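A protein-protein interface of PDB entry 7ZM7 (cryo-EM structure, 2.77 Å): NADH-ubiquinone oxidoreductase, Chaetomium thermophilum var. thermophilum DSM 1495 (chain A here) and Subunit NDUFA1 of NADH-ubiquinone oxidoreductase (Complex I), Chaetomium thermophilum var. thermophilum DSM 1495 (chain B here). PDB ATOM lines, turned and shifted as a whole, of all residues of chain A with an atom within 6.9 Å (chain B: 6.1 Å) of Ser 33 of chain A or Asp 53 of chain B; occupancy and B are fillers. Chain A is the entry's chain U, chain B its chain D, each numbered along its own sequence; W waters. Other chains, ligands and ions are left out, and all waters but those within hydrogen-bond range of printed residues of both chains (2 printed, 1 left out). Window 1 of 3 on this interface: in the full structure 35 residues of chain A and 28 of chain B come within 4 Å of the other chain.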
ATOM      1  N   ALA A  31      33.132  -1.853  18.095  1.00  0.00           N
ATOM      2  CA  ALA A  31      33.018  -2.782  19.200  1.00  0.00           C
ATOM      3  C   ALA A  31      32.011  -3.865  18.876  1.00  0.00           C
ATOM      4  O   ALA A  31      30.978  -3.618  18.249  1.00  0.00           O
ATOM      5  CB  ALA A  31      32.614  -2.058  20.473  1.00  0.00           C
ATOM      6  N   SER A  32      32.326  -5.075  19.307  1.00  0.00           N
ATOM      7  CA  SER A  32      31.480  -6.227  19.095  1.00  0.00           C
ATOM      8  C   SER A  32      30.375  -6.270  20.146  1.00  0.00           C
ATOM      9  O   SER A  32      30.235  -5.376  20.980  1.00  0.00           O
ATOM     10  CB  SER A  32      32.328  -7.488  19.106  1.00  0.00           C
ATOM     11  OG  SER A  32      31.535  -8.633  19.287  1.00  0.00           O
ATOM     12  N   SER A  33      29.581  -7.339  20.106  1.00  0.00           N
ATOM     13  CA  SER A  33      28.336  -7.377  20.866  1.00  0.00           C
ATOM     14  C   SER A  33      28.572  -7.319  22.368  1.00  0.00           C
ATOM     15  O   SER A  33      27.878  -6.587  23.077  1.00  0.00           O
ATOM     16  CB  SER A  33      27.542  -8.624  20.493  1.00  0.00           C
ATOM     17  OG  SER A  33      26.572  -8.903  21.469  1.00  0.00           O
ATOM     18  N   ALA A  34      29.539  -8.077  22.879  1.00  0.00           N
ATOM     19  CA  ALA A  34      29.754  -8.079  24.326  1.00  0.00           C
ATOM     20  C   ALA A  34      30.407  -6.796  24.819  1.00  0.00           C
ATOM     21  O   ALA A  34      29.945  -6.252  25.834  1.00  0.00           O
ATOM     22  CB  ALA A  34      30.538  -9.322  24.745  1.00  0.00           C
ATOM     23  N   PRO A  35      31.476  -6.229  24.193  1.00  0.00           N
ATOM     24  CA  PRO A  35      31.965  -4.902  24.583  1.00  0.00           C
ATOM     25  C   PRO A  35      30.836  -3.855  24.653  1.00  0.00           C
ATOM     26  O   PRO A  35      30.856  -3.064  25.553  1.00  0.00           O
ATOM     27  CB  PRO A  35      32.966  -4.567  23.479  1.00  0.00           C
ATOM     28  CG  PRO A  35      33.575  -5.888  23.145  1.00  0.00           C
ATOM     29  CD  PRO A  35      32.392  -6.823  23.192  1.00  0.00           C
ATOM     30  N   LEU A  36      29.861  -3.873  23.748  1.00  0.00           N
ATOM     31  CA  LEU A  36      28.726  -2.897  23.756  1.00  0.00           C
ATOM     32  C   LEU A  36      27.856  -3.037  25.014  1.00  0.00           C
ATOM     33  O   LEU A  36      27.520  -2.003  25.584  1.00  0.00           O
ATOM     34  CB  LEU A  36      27.895  -3.038  22.480  1.00  0.00           C
ATOM     35  CG  LEU A  36      28.508  -2.429  21.222  1.00  0.00           C
ATOM     36  CD1 LEU A  36      27.565  -2.594  20.042  1.00  0.00           C
ATOM     37  CD2 LEU A  36      28.842  -0.962  21.436  1.00  0.00           C
ATOM     38  N   LEU A  37      27.509  -4.256  25.431  1.00  0.00           N
ATOM     39  CA  LEU A  37      26.711  -4.489  26.658  1.00  0.00           C
ATOM     40  C   LEU A  37      27.464  -4.034  27.917  1.00  0.00           C
ATOM     41  O   LEU A  37      26.814  -3.524  28.829  1.00  0.00           O
ATOM     42  CB  LEU A  37      26.333  -5.970  26.717  1.00  0.00           C
ATOM     43  CG  LEU A  37      25.242  -6.327  27.719  1.00  0.00           C
ATOM     44  CD1 LEU A  37      23.946  -5.615  27.374  1.00  0.00           C
ATOM     45  CD2 LEU A  37      25.029  -7.828  27.762  1.00  0.00           C
ATOM     46  N   SER A  38      28.771  -4.263  27.988  1.00  0.00           N
ATOM     47  CA  SER A  38      29.571  -3.805  29.152  1.00  0.00           C
ATOM     48  C   SER A  38      29.534  -2.285  29.231  1.00  0.00           C
ATOM     49  O   SER A  38      29.438  -1.755  30.350  1.00  0.00           O
ATOM     50  CB  SER A  38      30.985  -4.279  29.052  1.00  0.00           C
ATOM     51  OG  SER A  38      31.088  -5.647  29.393  1.00  0.00           O
ATOM     52  N   TRP A  99      33.698  -7.948  29.806  1.00  0.00           N
ATOM     53  CA  TRP A  99      33.002  -8.323  28.545  1.00  0.00           C
ATOM     54  C   TRP A  99      33.422  -9.705  28.113  1.00  0.00           C
ATOM     55  O   TRP A  99      32.636 -10.369  27.443  1.00  0.00           O
ATOM     56  CB  TRP A  99      33.108  -7.290  27.413  1.00  0.00           C
ATOM     57  CG  TRP A  99      34.438  -6.998  26.788  1.00  0.00           C
ATOM     58  CD1 TRP A  99      35.156  -5.848  26.930  1.00  0.00           C
ATOM     59  CD2 TRP A  99      35.160  -7.797  25.833  1.00  0.00           C
ATOM     60  NE1 TRP A  99      36.290  -5.895  26.172  1.00  0.00           N
ATOM     61  CE2 TRP A  99      36.322  -7.078  25.488  1.00  0.00           C
ATOM     62  CE3 TRP A  99      34.951  -9.048  25.245  1.00  0.00           C
ATOM     63  CZ2 TRP A  99      37.274  -7.577  24.605  1.00  0.00           C
ATOM     64  CZ3 TRP A  99      35.893  -9.542  24.372  1.00  0.00           C
ATOM     65  CH2 TRP A  99      37.037  -8.814  24.053  1.00  0.00           C
ATOM     66  N   LEU A 102      31.075 -11.868  30.062  1.00  0.00           N
ATOM     67  CA  LEU A 102      29.759 -11.950  29.440  1.00  0.00           C
ATOM     68  C   LEU A 102      29.777 -12.851  28.221  1.00  0.00           C
ATOM     69  O   LEU A 102      28.754 -13.447  27.874  1.00  0.00           O
ATOM     70  CB  LEU A 102      29.271 -10.557  29.050  1.00  0.00           C
ATOM     71  CG  LEU A 102      29.121  -9.478  30.115  1.00  0.00           C
ATOM     72  CD1 LEU A 102      29.195  -8.150  29.463  1.00  0.00           C
ATOM     73  CD2 LEU A 102      27.815  -9.609  30.817  1.00  0.00           C
ATOM     74  N   ASP A 103      30.916 -12.960  27.549  1.00  0.00           N
ATOM     75  CA  ASP A 103      31.027 -13.885  26.388  1.00  0.00           C
ATOM     76  C   ASP A 103      30.661 -15.309  26.798  1.00  0.00           C
ATOM     77  O   ASP A 103      29.983 -15.986  26.016  1.00  0.00           O
ATOM     78  CB  ASP A 103      32.456 -14.001  25.864  1.00  0.00           C
ATOM     79  CG  ASP A 103      32.918 -12.818  25.050  1.00  0.00           C
ATOM     80  OD1 ASP A 103      32.084 -11.942  24.790  1.00  0.00           O
ATOM     81  OD2 ASP A 103      34.107 -12.790  24.685  1.00  0.00           O
ATOM     82  N   GLN A 107      25.915 -13.705  27.731  1.00  0.00           N
ATOM     83  CA  GLN A 107      25.804 -12.225  27.802  1.00  0.00           C
ATOM     84  C   GLN A 107      24.725 -11.850  28.811  1.00  0.00           C
ATOM     85  O   GLN A 107      24.080 -10.814  28.606  1.00  0.00           O
ATOM     86  CB  GLN A 107      25.597 -11.610  26.417  1.00  0.00           C
ATOM     87  CG  GLN A 107      26.902 -11.287  25.708  1.00  0.00           C
ATOM     88  CD  GLN A 107      26.676 -10.802  24.299  1.00  0.00           C
ATOM     89  OE1 GLN A 107      27.489 -11.027  23.408  1.00  0.00           O
ATOM     90  NE2 GLN A 107      25.550 -10.146  24.085  1.00  0.00           N
ATOM     91  N   ARG B  39      25.746 -20.012  23.312  1.00  0.00           N
ATOM     92  CA  ARG B  39      24.590 -19.141  23.638  1.00  0.00           C
ATOM     93  C   ARG B  39      23.344 -20.014  23.806  1.00  0.00           C
ATOM     94  O   ARG B  39      23.265 -21.042  23.137  1.00  0.00           O
ATOM     95  CB  ARG B  39      24.436 -18.089  22.537  1.00  0.00           C
ATOM     96  CG  ARG B  39      25.588 -17.101  22.454  1.00  0.00           C
ATOM     97  CD  ARG B  39      25.615 -16.220  23.681  1.00  0.00           C
ATOM     98  NE  ARG B  39      24.374 -15.471  23.777  1.00  0.00           N
ATOM     99  CZ  ARG B  39      24.240 -14.197  23.445  1.00  0.00           C
ATOM    100  NH1 ARG B  39      25.285 -13.515  23.018  1.00  0.00           N
ATOM    101  NH2 ARG B  39      23.069 -13.600  23.561  1.00  0.00           N
ATOM    102  N   ASP B  46      19.616 -11.134  19.683  1.00  0.00           N
ATOM    103  CA  ASP B  46      20.888 -11.844  19.965  1.00  0.00           C
ATOM    104  C   ASP B  46      21.466 -12.375  18.660  1.00  0.00           C
ATOM    105  O   ASP B  46      22.686 -12.308  18.483  1.00  0.00           O
ATOM    106  CB  ASP B  46      20.653 -12.986  20.955  1.00  0.00           C
ATOM    107  CG  ASP B  46      20.074 -12.538  22.283  1.00  0.00           C
ATOM    108  OD1 ASP B  46      20.358 -11.399  22.688  1.00  0.00           O
ATOM    109  OD2 ASP B  46      19.338 -13.333  22.894  1.00  0.00           O
ATOM    110  N   GLN B  48      20.987 -11.200  15.518  1.00  0.00           N
ATOM    111  CA  GLN B  48      21.509 -10.064  14.737  1.00  0.00           C
ATOM    112  C   GLN B  48      22.811  -9.573  15.361  1.00  0.00           C
ATOM    113  O   GLN B  48      23.712  -9.195  14.605  1.00  0.00           O
ATOM    114  CB  GLN B  48      20.451  -8.970  14.681  1.00  0.00           C
ATOM    115  CG  GLN B  48      19.190  -9.386  13.946  1.00  0.00           C
ATOM    116  CD  GLN B  48      18.131  -8.321  14.043  1.00  0.00           C
ATOM    117  OE1 GLN B  48      17.126  -8.356  13.343  1.00  0.00           O
ATOM    118  NE2 GLN B  48      18.360  -7.356  14.915  1.00  0.00           N
ATOM    119  N   GLN B  49      22.894  -9.562  16.687  1.00  0.00           N
ATOM    120  CA  GLN B  49      24.132  -9.130  17.374  1.00  0.00           C
ATOM    121  C   GLN B  49      25.283 -10.057  16.977  1.00  0.00           C
ATOM    122  O   GLN B  49      26.374  -9.547  16.702  1.00  0.00           O
ATOM    123  CB  GLN B  49      23.894  -9.010  18.878  1.00  0.00           C
ATOM    124  CG  GLN B  49      23.240  -7.706  19.298  1.00  0.00           C
ATOM    125  CD  GLN B  49      24.194  -6.539  19.240  1.00  0.00           C
ATOM    126  OE1 GLN B  49      25.276  -6.627  18.670  1.00  0.00           O
ATOM    127  NE2 GLN B  49      23.801  -5.431  19.839  1.00  0.00           N
ATOM    128  N   MET B  50      25.040 -11.357  16.917  1.00  0.00           N
ATOM    129  CA  MET B  50      26.058 -12.330  16.445  1.00  0.00           C
ATOM    130  C   MET B  50      26.378 -12.110  14.962  1.00  0.00           C
ATOM    131  O   MET B  50      27.532 -12.309  14.588  1.00  0.00           O
ATOM    132  CB  MET B  50      25.593 -13.761  16.679  1.00  0.00           C
ATOM    133  CG  MET B  50      25.808 -14.223  18.103  1.00  0.00           C
ATOM    134  SD  MET B  50      25.398 -15.963  18.342  1.00  0.00           S
ATOM    135  CE  MET B  50      23.611 -15.885  18.295  1.00  0.00           C
ATOM    136  N   GLU B  51      25.396 -11.748  14.148  1.00  0.00           N
ATOM    137  CA  GLU B  51      25.642 -11.439  12.719  1.00  0.00           C
ATOM    138  C   GLU B  51      26.590 -10.245  12.576  1.00  0.00           C
ATOM    139  O   GLU B  51      27.372 -10.240  11.630  1.00  0.00           O
ATOM    140  CB  GLU B  51      24.319 -11.335  11.965  1.00  0.00           C
ATOM    141  CG  GLU B  51      23.795 -12.689  11.551  1.00  0.00           C
ATOM    142  CD  GLU B  51      22.582 -12.667  10.645  1.00  0.00           C
ATOM    143  OE1 GLU B  51      22.326 -11.618  10.023  1.00  0.00           O
ATOM    144  OE2 GLU B  51      21.892 -13.698  10.578  1.00  0.00           O
ATOM    145  N   ARG B  52      26.501  -9.269  13.470  1.00  0.00           N
ATOM    146  CA  ARG B  52      27.345  -8.060  13.365  1.00  0.00           C
ATOM    147  C   ARG B  52      28.689  -8.450  13.950  1.00  0.00           C
ATOM    148  O   ARG B  52      29.690  -7.830  13.581  1.00  0.00           O
ATOM    149  CB  ARG B  52      26.681  -6.885  14.079  1.00  0.00           C
ATOM    150  CG  ARG B  52      27.488  -5.596  14.078  1.00  0.00           C
ATOM    151  CD  ARG B  52      26.840  -4.569  14.979  1.00  0.00           C
ATOM    152  NE  ARG B  52      27.474  -3.274  14.823  1.00  0.00           N
ATOM    153  CZ  ARG B  52      28.306  -2.736  15.701  1.00  0.00           C
ATOM    154  NH1 ARG B  52      28.590  -3.379  16.819  1.00  0.00           N
ATOM    155  NH2 ARG B  52      28.833  -1.550  15.465  1.00  0.00           N
ATOM    156  N   ASP B  53      28.705  -9.445  14.839  1.00  0.00           N
ATOM    157  CA  ASP B  53      29.997  -9.959  15.272  1.00  0.00           C
ATOM    158  C   ASP B  53      30.733 -10.607  14.120  1.00  0.00           C
ATOM    159  O   ASP B  53      31.954 -10.481  14.007  1.00  0.00           O
ATOM    160  CB  ASP B  53      29.814 -10.979  16.389  1.00  0.00           C
ATOM    161  CG  ASP B  53      29.240 -10.384  17.632  1.00  0.00           C
ATOM    162  OD1 ASP B  53      28.992  -9.165  17.649  1.00  0.00           O
ATOM    163  OD2 ASP B  53      29.045 -11.141  18.604  1.00  0.00           O
ATOM    164  N   ARG B  54      30.006 -11.338  13.274  1.00  0.00           N
ATOM    165  CA  ARG B  54      30.605 -11.914  12.081  1.00  0.00           C
ATOM    166  C   ARG B  54      31.098 -10.834  11.146  1.00  0.00           C
ATOM    167  O   ARG B  54      32.143 -10.991  10.516  1.00  0.00           O
ATOM    168  CB  ARG B  54      29.607 -12.812  11.364  1.00  0.00           C
ATOM    169  CG  ARG B  54      30.179 -13.474  10.130  1.00  0.00           C
ATOM    170  CD  ARG B  54      29.556 -14.807   9.891  1.00  0.00           C
ATOM    171  NE  ARG B  54      28.145 -14.666   9.600  1.00  0.00           N
ATOM    172  CZ  ARG B  54      27.335 -15.682   9.369  1.00  0.00           C
ATOM    173  NH1 ARG B  54      26.061 -15.468   9.112  1.00  0.00           N
ATOM    174  NH2 ARG B  54      27.806 -16.912   9.395  1.00  0.00           N
ATOM    175  N   ARG B  55      30.364  -9.730  11.058  1.00  0.00           N
ATOM    176  CA  ARG B  55      30.765  -8.629  10.200  1.00  0.00           C
ATOM    177  C   ARG B  55      32.091  -8.038  10.640  1.00  0.00           C
ATOM    178  O   ARG B  55      32.919  -7.671   9.804  1.00  0.00           O
ATOM    179  CB  ARG B  55      29.686  -7.555  10.192  1.00  0.00           C
ATOM    180  CG  ARG B  55      28.553  -7.848   9.275  1.00  0.00           C
ATOM    181  CD  ARG B  55      27.492  -6.812   9.402  1.00  0.00           C
ATOM    182  NE  ARG B  55      27.884  -5.580   8.750  1.00  0.00           N
ATOM    183  CZ  ARG B  55      27.641  -4.371   9.228  1.00  0.00           C
ATOM    184  NH1 ARG B  55      27.011  -4.231  10.378  1.00  0.00           N
ATOM    185  NH2 ARG B  55      28.035  -3.304   8.558  1.00  0.00           N
ATOM    186  N   LEU B  56      32.304  -7.914  11.943  1.00  0.00           N
ATOM    187  CA  LEU B  56      33.532  -7.290  12.412  1.00  0.00           C
ATOM    188  C   LEU B  56      34.699  -8.265  12.431  1.00  0.00           C
ATOM    189  O   LEU B  56      35.828  -7.878  12.126  1.00  0.00           O
ATOM    190  CB  LEU B  56      33.314  -6.682  13.795  1.00  0.00           C
ATOM    191  CG  LEU B  56      32.488  -5.406  13.788  1.00  0.00           C
ATOM    192  CD1 LEU B  56      31.922  -5.130  15.156  1.00  0.00           C
ATOM    193  CD2 LEU B  56      33.306  -4.245  13.311  1.00  0.00           C
ATOM    194  N   THR B  57      34.456  -9.524  12.766  1.00  0.00           N
ATOM    195  CA  THR B  57      35.526 -10.496  12.932  1.00  0.00           C
ATOM    196  C   THR B  57      35.519 -11.631  11.922  1.00  0.00           C
ATOM    197  O   THR B  57      36.574 -12.202  11.663  1.00  0.00           O
ATOM    198  CB  THR B  57      35.480 -11.118  14.331  1.00  0.00           C
ATOM    199  OG1 THR B  57      34.436 -12.090  14.377  1.00  0.00           O
ATOM    200  CG2 THR B  57      35.247 -10.054  15.389  1.00  0.00           C
ATOM    201  N   GLY B  58      34.352 -12.038  11.430  1.00  0.00           N
ATOM    202  CA  GLY B  58      34.256 -13.220  10.547  1.00  0.00           C
ATOM    203  C   GLY B  58      33.679 -14.407  11.295  1.00  0.00           C
ATOM    204  O   GLY B  58      33.181 -15.321  10.638  1.00  0.00           O
ATOM    205  N   HIS B  59      33.697 -14.361  12.627  1.00  0.00           N
ATOM    206  CA  HIS B  59      33.137 -15.447  13.473  1.00  0.00           C
ATOM    207  C   HIS B  59      31.876 -14.929  14.166  1.00  0.00           C
ATOM    208  O   HIS B  59      31.915 -13.811  14.680  1.00  0.00           O
ATOM    209  CB  HIS B  59      34.217 -15.944  14.439  1.00  0.00           C
ATOM    210  CG  HIS B  59      33.867 -17.138  15.262  1.00  0.00           C
ATOM    211  ND1 HIS B  59      32.718 -17.877  15.070  1.00  0.00           N
ATOM    212  CD2 HIS B  59      34.526 -17.734  16.278  1.00  0.00           C
ATOM    213  CE1 HIS B  59      32.681 -18.867  15.937  1.00  0.00           C
ATOM    214  NE2 HIS B  59      33.779 -18.804  16.685  1.00  0.00           N
ATOM    215  N   LEU B  60      30.809 -15.723  14.181  1.00  0.00           N
ATOM    216  CA  LEU B  60      29.533 -15.338  14.838  1.00  0.00           C
ATOM    217  C   LEU B  60      29.768 -15.116  16.332  1.00  0.00           C
ATOM    218  O   LEU B  60      29.050 -14.286  16.907  1.00  0.00           O
ATOM    219  CB  LEU B  60      28.499 -16.439  14.587  1.00  0.00           C
ATOM    220  CG  LEU B  60      27.897 -16.484  13.187  1.00  0.00           C
ATOM    221  CD1 LEU B  60      27.318 -17.857  12.896  1.00  0.00           C
ATOM    222  CD2 LEU B  60      26.833 -15.411  13.023  1.00  0.00           C
ATOM    223  N   ARG B  61      30.711 -15.843  16.939  1.00  0.00           N
ATOM    224  CA  ARG B  61      31.052 -15.633  18.371  1.00  0.00           C
ATOM    225  C   ARG B  61      32.235 -14.674  18.572  1.00  0.00           C
ATOM    226  O   ARG B  61      32.612 -14.481  19.738  1.00  0.00           O
ATOM    227  CB  ARG B  61      31.313 -16.967  19.065  1.00  0.00           C
ATOM    228  CG  ARG B  61      30.143 -17.937  19.007  1.00  0.00           C
ATOM    229  CD  ARG B  61      28.902 -17.359  19.655  1.00  0.00           C
ATOM    230  NE  ARG B  61      29.176 -16.831  20.982  1.00  0.00           N
ATOM    231  CZ  ARG B  61      29.113 -17.539  22.102  1.00  0.00           C
ATOM    232  NH1 ARG B  61      29.379 -16.968  23.261  1.00  0.00           N
ATOM    233  NH2 ARG B  61      28.786 -18.815  22.057  1.00  0.00           N
ATOM    234  N   GLY B  62      32.798 -14.089  17.514  1.00  0.00           N
ATOM    235  CA  GLY B  62      33.993 -13.230  17.665  1.00  0.00           C
ATOM    236  C   GLY B  62      33.733 -11.927  18.407  1.00  0.00           C
ATOM    237  O   GLY B  62      32.664 -11.345  18.181  1.00  0.00           O
ATOM    238  N   GLN B  63      34.683 -11.466  19.240  1.00  0.00           N
ATOM    239  CA  GLN B  63      34.521 -10.246  20.019  1.00  0.00           C
ATOM    240  C   GLN B  63      35.736  -9.350  19.856  1.00  0.00           C
ATOM    241  O   GLN B  63      36.867  -9.831  19.883  1.00  0.00           O
ATOM    242  CB  GLN B  63      34.305 -10.564  21.501  1.00  0.00           C
ATOM    243  CG  GLN B  63      33.102 -11.407  21.791  1.00  0.00           C
ATOM    244  CD  GLN B  63      31.843 -10.652  21.571  1.00  0.00           C
ATOM    245  OE1 GLN B  63      31.855  -9.436  21.514  1.00  0.00           O
ATOM    246  NE2 GLN B  63      30.744 -11.359  21.430  1.00  0.00           N
ATOM    247  N   THR B  64      35.495  -8.052  19.699  1.00  0.00           N
ATOM    248  CA  THR B  64      36.561  -7.031  19.524  1.00  0.00           C
ATOM    249  C   THR B  64      36.126  -5.752  20.232  1.00  0.00           C
ATOM    250  O   THR B  64      34.997  -5.311  20.015  1.00  0.00           O
ATOM    251  CB  THR B  64      36.687  -6.596  18.061  1.00  0.00           C
ATOM    252  OG1 THR B  64      35.398  -6.287  17.533  1.00  0.00           O
ATOM    253  CG2 THR B  64      37.367  -7.630  17.191  1.00  0.00           C
HETATM  254  O   HOH W   1      28.705 -13.743  24.052  1.00  0.00           O
HETATM  255  O   HOH W   2      22.965 -10.210  22.676  1.00  0.00           O
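Leu 56 of chain B touches Ala 31 of chain A. Thr 64 of chain B touches Ala 31 of chain A. Ser 33 of chain A touches Gln 49 of chain B (CB to OE1, 3.5 Å). Pro 35 of chain A touches Gln 63 of chain B. Pro 35 of chain A touches Thr 64 of chain B. NH1 of Arg 52 of chain B touches CD1 of Leu 36 of chain A, 3.5 Å away. Gln 63 of chain B touches Trp 99 of chain A. OD1 of Asp 103 of chain A touches CG of Gln 63 of chain B, 3.2 Å away. Gln 107 of chain A touches Gln 63 of chain B (OE1 to NE2, 3.8 Å).
OD1 of Asp 46 of chain B lies within salt-bridge range of NH2 of Arg 39 of chain B (3.6 Å). OG1 of Thr 57 of chain B lies within hydrogen-bond range of O of Asp 53 of chain B (3.0 Å). NE2 of Gln 63 of chain B lies within hydrogen-bond range of OD2 of Asp 53 of chain B (3.3 Å). A ring nitrogen (ND1) of His 59 of chain B lies close to the backbone NH (N) of Arg 61 of chain B (3.4 Å). The side-chain hydroxyl of Ser 33 of chain A is in hydrogen-bond range of the side-chain amide oxygen of Gln 107 of chain A, 3.0 Å away. The backbone carbonyl oxygen (O) of Leu 102 of chain A is in hydrogen-bond range of the backbone NH (N) of Gln 107 of chain A (2.9 Å).
Ser 33 of chain A touches three residues of chain B. Of chain A, only Ser 32 and Ser 33 come within 4 Å of Asp 53 of chain B. Printed residues of chain B within 4 Å of Trp 99 of chain A: Gln 63. Printed residues of chain B within 4 Å of Ala 31 of chain A: Arg 52 (2.8 Å), Leu 56 (3.6 Å) and Thr 64 (3.3 Å). Of the printed residues of chain A, Gln 63 of chain B touches Ser 32 (2.4 Å), Ser 33 (3.4 Å), Ala 34 (3.0 Å), Pro 35 (3.2 Å), Trp 99 (3.4 Å), Asp 103 (3.2 Å) and Gln 107 (3.8 Å). Of the printed residues of chain B, Ser 32 of chain A touches Asp 53 (3.1 Å), Gly 62 (3.1 Å), Gln 63 (2.4 Å) and Thr 64 (2.8 Å). Of the printed residues of chain A, Arg 39 of chain B touches Gln 107 (3.3 Å). His 59 of chain B touches none of the printed residues of chain A. Leu 60 of chain B touches none of the printed residues of chain A. The nearest residue of chain A that does not touch Asp 53 of chain B is Gln 107 of chain A (5.1 Å). The nearest printed residue of chain B that does not touch Leu 36 of chain A is Gln 49 of chain B (4.7 Å).
Of the 12 printed residues of chain A, 9 touch a printed residue of chain B. Hydrophobic or aromatic side chains of chain A within 4 Å of the printed part of chain B: Ala 34, Pro 35, Leu 36 and Trp 99. Of the 19 printed residues of chain B, 9 touch a printed residue of chain A. Printed residues of chain B that touch a printed residue of chain A: Arg 39, Gln 49, Arg 52, Asp 53, Leu 56, Arg 61, Gly 62, Gln 63 and Thr 64. Along chain B the printed residues that touch a printed residue of chain A span positions 39 to 64.
Water W2 bridges OD1 of Asp 46 of chain B (2.9 Å) and NE2 of Gln 107 of chain A (2.9 Å). Water W1 lies within hydrogen-bond range of OE1 of Gln 107 of chain A, O of Asp 103 of chain A and NH1 of Arg 61 of chain B.
The guanidinium group (NH1) of Arg 39 of chain B lies close to the side-chain amide oxygen (OE1) of Gln 107 of chain A (3.3 Å). The guanidinium group (NH1) of Arg 52 of chain B lies within hydrogen-bond range of the backbone carbonyl oxygen (O) of Ala 31 of chain A, at 2.8 Å. The side-chain carboxylate (OD1) of Asp 53 of chain B lies within hydrogen-bond range of the side-chain hydroxyl (OG) of Ser 32 of chain A, at 3.1 Å. The side-chain carboxylate (OD1) of Asp 53 of chain B sits at hydrogen-bond distance from the backbone NH (N) of Ser 33 of chain A (3.1 Å). The guanidinium group (NH1) of Arg 61 of chain B is in hydrogen-bond range of the backbone carbonyl oxygen (O) of Asp 103 of chain A (3.0 Å). OG of Ser 32 of chain A is in hydrogen-bond range of O of Gly 62 of chain B. The side-chain amide oxygen (OE1) of Gln 63 of chain B lies within hydrogen-bond range of the backbone NH (N) of Ser 33 of chain A (3.4 Å). The side-chain amide oxygen of Gln 63 of chain B is in hydrogen-bond range of the backbone NH of Ala 34 of chain A, at 3.0 Å. The backbone carbonyl oxygen (O) of Thr 64 of chain B sits at hydrogen-bond distance from the backbone NH (N) of Ser 32 of chain A, at 2.8 Å. OG of Ser 32 of chain A sits close to OE1 of Gln 63 of chain B (2.4 Å).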
